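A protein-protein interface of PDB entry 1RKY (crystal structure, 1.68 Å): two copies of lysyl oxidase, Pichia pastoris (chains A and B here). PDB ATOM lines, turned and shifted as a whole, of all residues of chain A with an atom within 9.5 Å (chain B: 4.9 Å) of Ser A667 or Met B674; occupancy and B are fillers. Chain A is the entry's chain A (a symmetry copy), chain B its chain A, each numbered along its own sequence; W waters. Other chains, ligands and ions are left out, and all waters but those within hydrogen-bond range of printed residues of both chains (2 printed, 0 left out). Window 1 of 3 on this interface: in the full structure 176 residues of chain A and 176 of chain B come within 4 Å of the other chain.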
ATOM      1  N   ASN A 441      -7.451   5.662 -10.354  1.00  0.00           N
ATOM      2  CA  ASN A 441      -8.453   6.478  -9.721  1.00  0.00           C
ATOM      3  C   ASN A 441      -8.665   5.885  -8.330  1.00  0.00           C
ATOM      4  O   ASN A 441      -9.187   4.794  -8.198  1.00  0.00           O
ATOM      5  CB  ASN A 441      -9.709   6.429 -10.568  1.00  0.00           C
ATOM      6  CG  ASN A 441     -10.789   7.312 -10.093  1.00  0.00           C
ATOM      7  OD1 ASN A 441     -10.880   7.671  -8.896  1.00  0.00           O
ATOM      8  ND2 ASN A 441     -11.677   7.684 -11.036  1.00  0.00           N
ATOM      9  N   VAL A 456     -10.026   1.205  -5.857  1.00  0.00           N
ATOM     10  CA  VAL A 456      -9.223   1.670  -6.957  1.00  0.00           C
ATOM     11  C   VAL A 456      -9.889   1.216  -8.258  1.00  0.00           C
ATOM     12  O   VAL A 456     -10.464   0.141  -8.322  1.00  0.00           O
ATOM     13  CB  VAL A 456      -7.773   1.210  -6.839  1.00  0.00           C
ATOM     14  CG1 VAL A 456      -7.631  -0.304  -6.818  1.00  0.00           C
ATOM     15  CG2 VAL A 456      -6.941   1.803  -7.974  1.00  0.00           C
ATOM     16  N   ARG A 457      -9.836   2.073  -9.276  1.00  0.00           N
ATOM     17  CA  ARG A 457     -10.212   1.706 -10.645  1.00  0.00           C
ATOM     18  C   ARG A 457      -9.090   2.140 -11.588  1.00  0.00           C
ATOM     19  O   ARG A 457      -8.340   3.070 -11.302  1.00  0.00           O
ATOM     20  CB  ARG A 457     -11.481   2.423 -11.043  1.00  0.00           C
ATOM     21  CG  ARG A 457     -12.726   2.081 -10.136  1.00  0.00           C
ATOM     22  CD  ARG A 457     -13.948   2.925 -10.455  1.00  0.00           C
ATOM     23  NE  ARG A 457     -15.120   2.579  -9.637  1.00  0.00           N
ATOM     24  CZ  ARG A 457     -15.943   1.551  -9.859  1.00  0.00           C
ATOM     25  NH1 ARG A 457     -15.782   0.696 -10.870  1.00  0.00           N
ATOM     26  NH2 ARG A 457     -16.978   1.384  -9.035  1.00  0.00           N
ATOM     27  N   ALA A 458      -9.000   1.459 -12.708  1.00  0.00           N
ATOM     28  CA  ALA A 458      -7.938   1.722 -13.675  1.00  0.00           C
ATOM     29  C   ALA A 458      -8.540   1.974 -15.046  1.00  0.00           C
ATOM     30  O   ALA A 458      -9.582   1.418 -15.421  1.00  0.00           O
ATOM     31  CB  ALA A 458      -7.007   0.578 -13.722  1.00  0.00           C
ATOM     32  N   ALA A 459      -7.871   2.839 -15.795  1.00  0.00           N
ATOM     33  CA  ALA A 459      -8.278   3.163 -17.157  1.00  0.00           C
ATOM     34  C   ALA A 459      -7.001   3.561 -17.907  1.00  0.00           C
ATOM     35  O   ALA A 459      -5.903   3.362 -17.393  1.00  0.00           O
ATOM     36  CB  ALA A 459      -9.312   4.293 -17.184  1.00  0.00           C
ATOM     37  N   GLY A 460      -7.148   4.070 -19.115  1.00  0.00           N
ATOM     38  CA  GLY A 460      -6.000   4.464 -19.909  1.00  0.00           C
ATOM     39  C   GLY A 460      -5.659   3.490 -21.020  1.00  0.00           C
ATOM     40  O   GLY A 460      -6.486   2.699 -21.429  1.00  0.00           O
ATOM     41  N   LEU A 652      -6.010  -6.980  -9.984  1.00  0.00           N
ATOM     42  CA  LEU A 652      -6.753  -7.301 -11.187  1.00  0.00           C
ATOM     43  C   LEU A 652      -5.877  -8.151 -12.080  1.00  0.00           C
ATOM     44  O   LEU A 652      -4.739  -7.749 -12.330  1.00  0.00           O
ATOM     45  CB  LEU A 652      -7.096  -6.022 -11.933  1.00  0.00           C
ATOM     46  CG  LEU A 652      -7.705  -6.184 -13.334  1.00  0.00           C
ATOM     47  CD1 LEU A 652      -9.006  -6.953 -13.259  1.00  0.00           C
ATOM     48  CD2 LEU A 652      -7.898  -4.827 -14.065  1.00  0.00           C
ATOM     49  N   ASN A 659     -12.944  -4.488 -25.514  1.00  0.00           N
ATOM     50  CA  ASN A 659     -13.480  -3.483 -24.602  1.00  0.00           C
ATOM     51  C   ASN A 659     -12.406  -2.695 -23.888  1.00  0.00           C
ATOM     52  O   ASN A 659     -12.733  -1.833 -23.062  1.00  0.00           O
ATOM     53  CB  ASN A 659     -14.446  -4.126 -23.579  1.00  0.00           C
ATOM     54  CG  ASN A 659     -15.784  -3.416 -23.520  1.00  0.00           C
ATOM     55  OD1 ASN A 659     -16.396  -3.180 -24.557  1.00  0.00           O
ATOM     56  ND2 ASN A 659     -16.265  -3.126 -22.314  1.00  0.00           N
ATOM     57  N   ASP A 660     -11.142  -2.918 -24.261  1.00  0.00           N
ATOM     58  CA  ASP A 660     -10.025  -2.098 -23.809  1.00  0.00           C
ATOM     59  C   ASP A 660      -9.416  -1.238 -24.937  1.00  0.00           C
ATOM     60  O   ASP A 660      -8.353  -0.641 -24.736  1.00  0.00           O
ATOM     61  CB  ASP A 660      -8.933  -2.973 -23.215  1.00  0.00           C
ATOM     62  CG  ASP A 660      -9.399  -3.742 -21.979  1.00  0.00           C
ATOM     63  OD1 ASP A 660      -9.366  -3.165 -20.876  1.00  0.00           O
ATOM     64  OD2 ASP A 660      -9.801  -4.913 -22.041  1.00  0.00           O
ATOM     65  N   ASN A 663      -9.260   2.542 -25.071  1.00  0.00           N
ATOM     66  CA  ASN A 663      -8.811   2.613 -23.665  1.00  0.00           C
ATOM     67  C   ASN A 663      -9.589   1.604 -22.813  1.00  0.00           C
ATOM     68  O   ASN A 663     -10.731   1.272 -23.112  1.00  0.00           O
ATOM     69  CB  ASN A 663      -9.125   3.993 -23.062  1.00  0.00           C
ATOM     70  CG  ASN A 663      -7.974   4.973 -23.065  1.00  0.00           C
ATOM     71  OD1 ASN A 663      -8.009   5.916 -22.281  1.00  0.00           O
ATOM     72  ND2 ASN A 663      -6.996   4.810 -23.955  1.00  0.00           N
ATOM     73  N   THR A 664      -8.945   1.158 -21.733  1.00  0.00           N
ATOM     74  CA  THR A 664      -9.600   0.467 -20.655  1.00  0.00           C
ATOM     75  C   THR A 664     -10.603   1.367 -19.920  1.00  0.00           C
ATOM     76  O   THR A 664     -10.346   2.557 -19.756  1.00  0.00           O
ATOM     77  CB  THR A 664      -8.493   0.008 -19.683  1.00  0.00           C
ATOM     78  OG1 THR A 664      -7.679  -0.988 -20.330  1.00  0.00           O
ATOM     79  CG2 THR A 664      -9.096  -0.680 -18.467  1.00  0.00           C
ATOM     80  N   ILE A 665     -11.724   0.800 -19.457  1.00  0.00           N
ATOM     81  CA  ILE A 665     -12.766   1.575 -18.760  1.00  0.00           C
ATOM     82  C   ILE A 665     -12.778   1.277 -17.247  1.00  0.00           C
ATOM     83  O   ILE A 665     -12.435   0.201 -16.819  1.00  0.00           O
ATOM     84  CB  ILE A 665     -14.160   1.370 -19.413  1.00  0.00           C
ATOM     85  CG1 ILE A 665     -14.701  -0.034 -19.193  1.00  0.00           C
ATOM     86  CG2 ILE A 665     -14.066   1.685 -20.903  1.00  0.00           C
ATOM     87  CD1 ILE A 665     -16.070  -0.226 -19.691  1.00  0.00           C
ATOM     88  N   PHE A 666     -13.073   2.307 -16.466  1.00  0.00           N
ATOM     89  CA  PHE A 666     -13.034   2.267 -15.010  1.00  0.00           C
ATOM     90  C   PHE A 666     -14.123   1.367 -14.409  1.00  0.00           C
ATOM     91  O   PHE A 666     -13.964   0.850 -13.311  1.00  0.00           O
ATOM     92  CB  PHE A 666     -13.273   3.690 -14.450  1.00  0.00           C
ATOM     93  CG  PHE A 666     -12.074   4.587 -14.453  1.00  0.00           C
ATOM     94  CD1 PHE A 666     -12.199   5.923 -14.844  1.00  0.00           C
ATOM     95  CD2 PHE A 666     -10.867   4.163 -13.985  1.00  0.00           C
ATOM     96  CE1 PHE A 666     -11.118   6.785 -14.791  1.00  0.00           C
ATOM     97  CE2 PHE A 666      -9.772   5.037 -13.932  1.00  0.00           C
ATOM     98  CZ  PHE A 666      -9.907   6.336 -14.334  1.00  0.00           C
ATOM     99  N   SER A 667     -15.237   1.213 -15.100  1.00  0.00           N
ATOM    100  CA  SER A 667     -16.381   0.497 -14.568  1.00  0.00           C
ATOM    101  C   SER A 667     -16.085  -0.974 -14.267  1.00  0.00           C
ATOM    102  O   SER A 667     -16.529  -1.536 -13.249  1.00  0.00           O
ATOM    103  CB  SER A 667     -17.551   0.601 -15.547  1.00  0.00           C
ATOM    104  OG  SER A 667     -17.184   0.079 -16.818  1.00  0.00           O
ATOM    105  N   THR A 668     -15.310  -1.599 -15.137  1.00  0.00           N
ATOM    106  CA  THR A 668     -14.995  -3.039 -14.988  1.00  0.00           C
ATOM    107  C   THR A 668     -13.576  -3.373 -14.521  1.00  0.00           C
ATOM    108  O   THR A 668     -13.197  -4.540 -14.463  1.00  0.00           O
ATOM    109  CB  THR A 668     -15.306  -3.767 -16.324  1.00  0.00           C
ATOM    110  OG1 THR A 668     -14.781  -3.034 -17.437  1.00  0.00           O
ATOM    111  CG2 THR A 668     -16.785  -3.773 -16.611  1.00  0.00           C
ATOM    112  N   ALA A 669     -12.769  -2.356 -14.265  1.00  0.00           N
ATOM    113  CA  ALA A 669     -11.405  -2.512 -13.782  1.00  0.00           C
ATOM    114  C   ALA A 669     -11.370  -1.917 -12.372  1.00  0.00           C
ATOM    115  O   ALA A 669     -10.903  -0.799 -12.194  1.00  0.00           O
ATOM    116  CB  ALA A 669     -10.441  -1.788 -14.686  1.00  0.00           C
ATOM    117  N   HIS A 670     -11.892  -2.666 -11.411  1.00  0.00           N
ATOM    118  CA  HIS A 670     -12.252  -2.151 -10.087  1.00  0.00           C
ATOM    119  C   HIS A 670     -11.859  -3.134  -8.972  1.00  0.00           C
ATOM    120  O   HIS A 670     -11.989  -4.349  -9.128  1.00  0.00           O
ATOM    121  CB  HIS A 670     -13.746  -1.949 -10.042  1.00  0.00           C
ATOM    122  CG  HIS A 670     -14.259  -1.470  -8.730  1.00  0.00           C
ATOM    123  ND1 HIS A 670     -15.330  -2.053  -8.090  1.00  0.00           N
ATOM    124  CD2 HIS A 670     -13.858  -0.443  -7.939  1.00  0.00           C
ATOM    125  CE1 HIS A 670     -15.573  -1.402  -6.965  1.00  0.00           C
ATOM    126  NE2 HIS A 670     -14.696  -0.420  -6.848  1.00  0.00           N
ATOM    127  N   ALA A 671     -11.403  -2.603  -7.853  1.00  0.00           N
ATOM    128  CA  ALA A 671     -11.043  -3.419  -6.681  1.00  0.00           C
ATOM    129  C   ALA A 671     -11.363  -2.589  -5.431  1.00  0.00           C
ATOM    130  O   ALA A 671     -11.252  -1.353  -5.431  1.00  0.00           O
ATOM    131  CB  ALA A 671      -9.597  -3.760  -6.715  1.00  0.00           C
ATOM    132  N   TYR B 408     -17.762   8.066 -10.309  1.00  0.00           N
ATOM    133  CA  TYR B 408     -16.487   8.003 -11.011  1.00  0.00           C
ATOM    134  C   TYR B 408     -16.785   8.080 -12.513  1.00  0.00           C
ATOM    135  O   TYR B 408     -17.860   7.667 -12.974  1.00  0.00           O
ATOM    136  CB  TYR B 408     -15.743   6.677 -10.657  1.00  0.00           C
ATOM    137  CG  TYR B 408     -16.518   5.450 -11.112  1.00  0.00           C
ATOM    138  CD1 TYR B 408     -17.609   4.979 -10.396  1.00  0.00           C
ATOM    139  CD2 TYR B 408     -16.182   4.794 -12.301  1.00  0.00           C
ATOM    140  CE1 TYR B 408     -18.353   3.901 -10.850  1.00  0.00           C
ATOM    141  CE2 TYR B 408     -16.914   3.744 -12.743  1.00  0.00           C
ATOM    142  CZ  TYR B 408     -17.999   3.293 -12.032  1.00  0.00           C
ATOM    143  OH  TYR B 408     -18.704   2.225 -12.532  1.00  0.00           O
ATOM    144  N   LEU B 410     -16.473   7.172 -16.584  1.00  0.00           N
ATOM    145  CA  LEU B 410     -16.460   5.890 -17.265  1.00  0.00           C
ATOM    146  C   LEU B 410     -15.061   5.546 -17.751  1.00  0.00           C
ATOM    147  O   LEU B 410     -14.609   4.401 -17.654  1.00  0.00           O
ATOM    148  CB  LEU B 410     -17.480   5.867 -18.407  1.00  0.00           C
ATOM    149  CG  LEU B 410     -17.635   4.532 -19.141  1.00  0.00           C
ATOM    150  CD1 LEU B 410     -17.997   3.373 -18.150  1.00  0.00           C
ATOM    151  CD2 LEU B 410     -18.705   4.673 -20.199  1.00  0.00           C
ATOM    152  N   ASN B 424     -20.181   9.030 -16.604  1.00  0.00           N
ATOM    153  CA  ASN B 424     -20.715   7.691 -16.406  1.00  0.00           C
ATOM    154  C   ASN B 424     -22.165   7.728 -15.950  1.00  0.00           C
ATOM    155  O   ASN B 424     -22.499   7.309 -14.843  1.00  0.00           O
ATOM    156  CB  ASN B 424     -19.830   6.987 -15.371  1.00  0.00           C
ATOM    157  CG  ASN B 424     -19.976   5.506 -15.349  1.00  0.00           C
ATOM    158  OD1 ASN B 424     -20.687   4.897 -16.144  1.00  0.00           O
ATOM    159  ND2 ASN B 424     -19.244   4.876 -14.411  1.00  0.00           N
ATOM    160  N   PHE B 447     -24.967   0.428 -18.463  1.00  0.00           N
ATOM    161  CA  PHE B 447     -23.870   1.348 -18.755  1.00  0.00           C
ATOM    162  C   PHE B 447     -23.770   1.653 -20.241  1.00  0.00           C
ATOM    163  O   PHE B 447     -24.271   0.882 -21.089  1.00  0.00           O
ATOM    164  CB  PHE B 447     -22.531   0.798 -18.306  1.00  0.00           C
ATOM    165  CG  PHE B 447     -22.401   0.574 -16.796  1.00  0.00           C
ATOM    166  CD1 PHE B 447     -21.630   1.418 -16.031  1.00  0.00           C
ATOM    167  CD2 PHE B 447     -23.043  -0.491 -16.171  1.00  0.00           C
ATOM    168  CE1 PHE B 447     -21.484   1.188 -14.640  1.00  0.00           C
ATOM    169  CE2 PHE B 447     -22.891  -0.725 -14.794  1.00  0.00           C
ATOM    170  CZ  PHE B 447     -22.118   0.117 -14.037  1.00  0.00           C
ATOM    171  N   THR B 451     -22.462  -2.791 -20.882  1.00  0.00           N
ATOM    172  CA  THR B 451     -22.380  -3.583 -19.628  1.00  0.00           C
ATOM    173  C   THR B 451     -23.680  -3.423 -18.818  1.00  0.00           C
ATOM    174  O   THR B 451     -24.255  -2.334 -18.745  1.00  0.00           O
ATOM    175  CB  THR B 451     -21.148  -3.108 -18.781  1.00  0.00           C
ATOM    176  OG1 THR B 451     -19.918  -3.442 -19.472  1.00  0.00           O
ATOM    177  CG2 THR B 451     -21.016  -3.799 -17.425  1.00  0.00           C
ATOM    178  N   LEU B 452     -24.103  -4.503 -18.178  1.00  0.00           N
ATOM    179  CA  LEU B 452     -25.232  -4.520 -17.243  1.00  0.00           C
ATOM    180  C   LEU B 452     -24.738  -5.115 -15.913  1.00  0.00           C
ATOM    181  O   LEU B 452     -24.092  -6.153 -15.908  1.00  0.00           O
ATOM    182  CB  LEU B 452     -26.357  -5.405 -17.773  1.00  0.00           C
ATOM    183  CG  LEU B 452     -27.492  -5.810 -16.804  1.00  0.00           C
ATOM    184  CD1 LEU B 452     -28.220  -4.580 -16.237  1.00  0.00           C
ATOM    185  CD2 LEU B 452     -28.477  -6.745 -17.511  1.00  0.00           C
ATOM    186  N   GLU B 453     -25.110  -4.467 -14.815  1.00  0.00           N
ATOM    187  CA  GLU B 453     -24.808  -4.998 -13.479  1.00  0.00           C
ATOM    188  C   GLU B 453     -26.116  -5.318 -12.800  1.00  0.00           C
ATOM    189  O   GLU B 453     -27.022  -4.485 -12.722  1.00  0.00           O
ATOM    190  CB  GLU B 453     -24.049  -3.955 -12.659  1.00  0.00           C
ATOM    191  CG  GLU B 453     -23.651  -4.448 -11.271  1.00  0.00           C
ATOM    192  CD  GLU B 453     -23.235  -3.333 -10.311  1.00  0.00           C
ATOM    193  OE1 GLU B 453     -22.071  -3.352  -9.853  1.00  0.00           O
ATOM    194  OE2 GLU B 453     -24.058  -2.442  -9.990  1.00  0.00           O
ATOM    195  N   ASN B 573     -18.838 -11.606 -20.978  1.00  0.00           N
ATOM    196  CA  ASN B 573     -18.188 -12.146 -19.797  1.00  0.00           C
ATOM    197  C   ASN B 573     -19.176 -12.045 -18.637  1.00  0.00           C
ATOM    198  O   ASN B 573     -19.721 -10.958 -18.385  1.00  0.00           O
ATOM    199  CB  ASN B 573     -16.990 -11.254 -19.564  1.00  0.00           C
ATOM    200  CG  ASN B 573     -16.223 -11.522 -18.283  1.00  0.00           C
ATOM    201  OD1 ASN B 573     -15.505 -10.629 -17.830  1.00  0.00           O
ATOM    202  ND2 ASN B 573     -16.301 -12.724 -17.738  1.00  0.00           N
ATOM    203  N   ILE B 574     -19.396 -13.153 -17.937  1.00  0.00           N
ATOM    204  CA  ILE B 574     -20.120 -13.125 -16.667  1.00  0.00           C
ATOM    205  C   ILE B 574     -19.087 -12.965 -15.571  1.00  0.00           C
ATOM    206  O   ILE B 574     -18.319 -13.860 -15.324  1.00  0.00           O
ATOM    207  CB  ILE B 574     -20.922 -14.390 -16.469  1.00  0.00           C
ATOM    208  CG1 ILE B 574     -21.847 -14.647 -17.653  1.00  0.00           C
ATOM    209  CG2 ILE B 574     -21.718 -14.320 -15.180  1.00  0.00           C
ATOM    210  CD1 ILE B 574     -22.602 -15.989 -17.614  1.00  0.00           C
ATOM    211  N   MET B 575     -19.091 -11.795 -14.951  1.00  0.00           N
ATOM    212  CA  MET B 575     -18.043 -11.359 -14.044  1.00  0.00           C
ATOM    213  C   MET B 575     -18.640 -11.280 -12.645  1.00  0.00           C
ATOM    214  O   MET B 575     -19.544 -10.501 -12.413  1.00  0.00           O
ATOM    215  CB  MET B 575     -17.585  -9.981 -14.530  1.00  0.00           C
ATOM    216  CG  MET B 575     -16.470  -9.352 -13.687  1.00  0.00           C
ATOM    217  SD  MET B 575     -16.174  -7.560 -14.015  1.00  0.00           S
ATOM    218  CE  MET B 575     -16.639  -7.442 -15.685  1.00  0.00           C
ATOM    219  N   SER B 672     -23.443  -8.800  -6.226  1.00  0.00           N
ATOM    220  CA  SER B 672     -23.652  -8.356  -7.595  1.00  0.00           C
ATOM    221  C   SER B 672     -22.897  -9.236  -8.591  1.00  0.00           C
ATOM    222  O   SER B 672     -21.958  -9.940  -8.238  1.00  0.00           O
ATOM    223  CB  SER B 672     -23.195  -6.908  -7.769  1.00  0.00           C
ATOM    224  OG  SER B 672     -21.772  -6.762  -7.668  1.00  0.00           O
ATOM    225  N   PHE B 673     -23.320  -9.180  -9.841  1.00  0.00           N
ATOM    226  CA  PHE B 673     -22.520  -9.680 -10.963  1.00  0.00           C
ATOM    227  C   PHE B 673     -22.713  -8.741 -12.149  1.00  0.00           C
ATOM    228  O   PHE B 673     -23.659  -7.977 -12.182  1.00  0.00           O
ATOM    229  CB  PHE B 673     -22.848 -11.124 -11.360  1.00  0.00           C
ATOM    230  CG  PHE B 673     -24.242 -11.354 -11.870  1.00  0.00           C
ATOM    231  CD1 PHE B 673     -24.527 -11.287 -13.220  1.00  0.00           C
ATOM    232  CD2 PHE B 673     -25.266 -11.679 -11.002  1.00  0.00           C
ATOM    233  CE1 PHE B 673     -25.805 -11.509 -13.720  1.00  0.00           C
ATOM    234  CE2 PHE B 673     -26.538 -11.942 -11.480  1.00  0.00           C
ATOM    235  CZ  PHE B 673     -26.829 -11.829 -12.843  1.00  0.00           C
ATOM    236  N   MET B 674     -21.761  -8.778 -13.083  1.00  0.00           N
ATOM    237  CA  MET B 674     -21.814  -7.976 -14.281  1.00  0.00           C
ATOM    238  C   MET B 674     -21.810  -8.878 -15.520  1.00  0.00           C
ATOM    239  O   MET B 674     -21.263  -9.980 -15.507  1.00  0.00           O
ATOM    240  CB  MET B 674     -20.628  -7.023 -14.368  1.00  0.00           C
ATOM    241  CG  MET B 674     -20.862  -5.683 -13.695  1.00  0.00           C
ATOM    242  SD  MET B 674     -19.380  -4.660 -13.829  1.00  0.00           S
ATOM    243  CE  MET B 674     -20.038  -2.989 -13.413  1.00  0.00           C
ATOM    244  N   LEU B 675     -22.459  -8.388 -16.565  1.00  0.00           N
ATOM    245  CA  LEU B 675     -22.447  -8.959 -17.909  1.00  0.00           C
ATOM    246  C   LEU B 675     -21.774  -7.902 -18.754  1.00  0.00           C
ATOM    247  O   LEU B 675     -22.293  -6.804 -18.929  1.00  0.00           O
ATOM    248  CB  LEU B 675     -23.874  -9.240 -18.400  1.00  0.00           C
ATOM    249  CG  LEU B 675     -24.704 -10.158 -17.508  1.00  0.00           C
ATOM    250  CD1 LEU B 675     -26.073 -10.295 -18.100  1.00  0.00           C
ATOM    251  CD2 LEU B 675     -24.070 -11.526 -17.372  1.00  0.00           C
ATOM    252  N   THR B 676     -20.579  -8.203 -19.221  1.00  0.00           N
ATOM    253  CA  THR B 676     -19.795  -7.212 -19.921  1.00  0.00           C
ATOM    254  C   THR B 676     -19.299  -7.670 -21.293  1.00  0.00           C
ATOM    255  O   THR B 676     -18.882  -8.792 -21.467  1.00  0.00           O
ATOM    256  CB  THR B 676     -18.660  -6.690 -19.029  1.00  0.00           C
ATOM    257  OG1 THR B 676     -18.053  -5.537 -19.639  1.00  0.00           O
ATOM    258  CG2 THR B 676     -17.558  -7.690 -18.888  1.00  0.00           C
HETATM  259  O   HOH W   1     -15.475  -4.346 -19.873  1.00  0.00           O
HETATM  260  O   HOH W   2     -19.284  -0.388 -18.054  1.00  0.00           O
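Water W2 bridges OG of Ser A667 (2.5 Å) and OG1 of Thr B451 (3.4 Å). Water W1 lies within hydrogen-bond range of the side-chain amide nitrogen of Asn A659, the side-chain hydroxyl of Thr B676 and the side-chain hydroxyl of Thr A668.
Printed residues of chain A that touch a printed residue of chain B: Arg A457, Ile A665, Phe A666, Ser A667 and Thr A668. Hydrophobic or aromatic side chains of chain A within 4 Å of the printed part of chain B: Ile A665 and Phe A666. Along chain A the printed residues that touch a printed residue of chain B span positions 457 to 668. Of the 15 printed residues of chain B, 5 touch a printed residue of chain A.
The backbone carbonyl oxygen (O) of Thr B676 lies within hydrogen-bond range of the backbone NH (N) of Asn B573, at 2.9 Å. The guanidinium group of Arg A457 sits at hydrogen-bond distance from the backbone carbonyl oxygen of Phe A666, 3.0 Å away. The backbone NH of Met B575 sits at hydrogen-bond distance from the backbone carbonyl oxygen of Met B674, 2.9 Å away. The guanidinium group of Arg A457 lies within hydrogen-bond range of the backbone carbonyl oxygen of Ser A667, 3.3 Å away. The side-chain amide nitrogen of Asn B424 lies close to the side-chain hydroxyl of Tyr B408 (3.3 Å). The backbone carbonyl oxygen (O) of Arg A457 lies within hydrogen-bond range of the backbone NH (N) of Asn A441.
Arg A457 touches Tyr B408 (NH2 to CE1, 3.4 Å). Ile A665 touches Leu B410. Phe A666 touches Tyr B408 (CB to CD2, 3.8 Å). Ser A667 touches Tyr B408. Ser A667 touches Leu B410 (OG to CD1, 3.6 Å). Ser A667 touches Met B674 (O to CE, 3.8 Å). Thr A668 touches Met B575 (CG2 to CE, 3.8 Å). SD of Met B674 touches CG2 of Thr A668, at 3.9 Å. Thr A668 touches Thr B676.
Of the printed residues of chain B, Arg A457 touches Tyr B408 (3.4 Å). Printed residues of chain B within 4 Å of Phe A666: Tyr B408 (3.8 Å) and Leu B410 (2.9 Å). Ser A667 touches three residues of chain B. Of the printed residues of chain B, Thr A668 touches Met B575, Met B674 and Thr B676. Printed residues of chain A within 4 Å of Tyr B408: Arg A457 (3.4 Å), Phe A666 (3.8 Å) and Ser A667 (3.5 Å). Of the printed residues of chain A, Met B674 touches Ser A667 and Thr A668. No residue of chain A comes within 4 Å of Leu B675. Of the printed residues of chain A, Thr B676 touches Thr A668. The nearest residue of chain A that does not touch Met B674 is Arg A457 (6.2 Å).
No position is printed for both chains.
The backbone carbonyl oxygen (O) of Leu B410 lies within hydrogen-bond range of the backbone NH (N) of Phe A666, at 2.9 Å.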
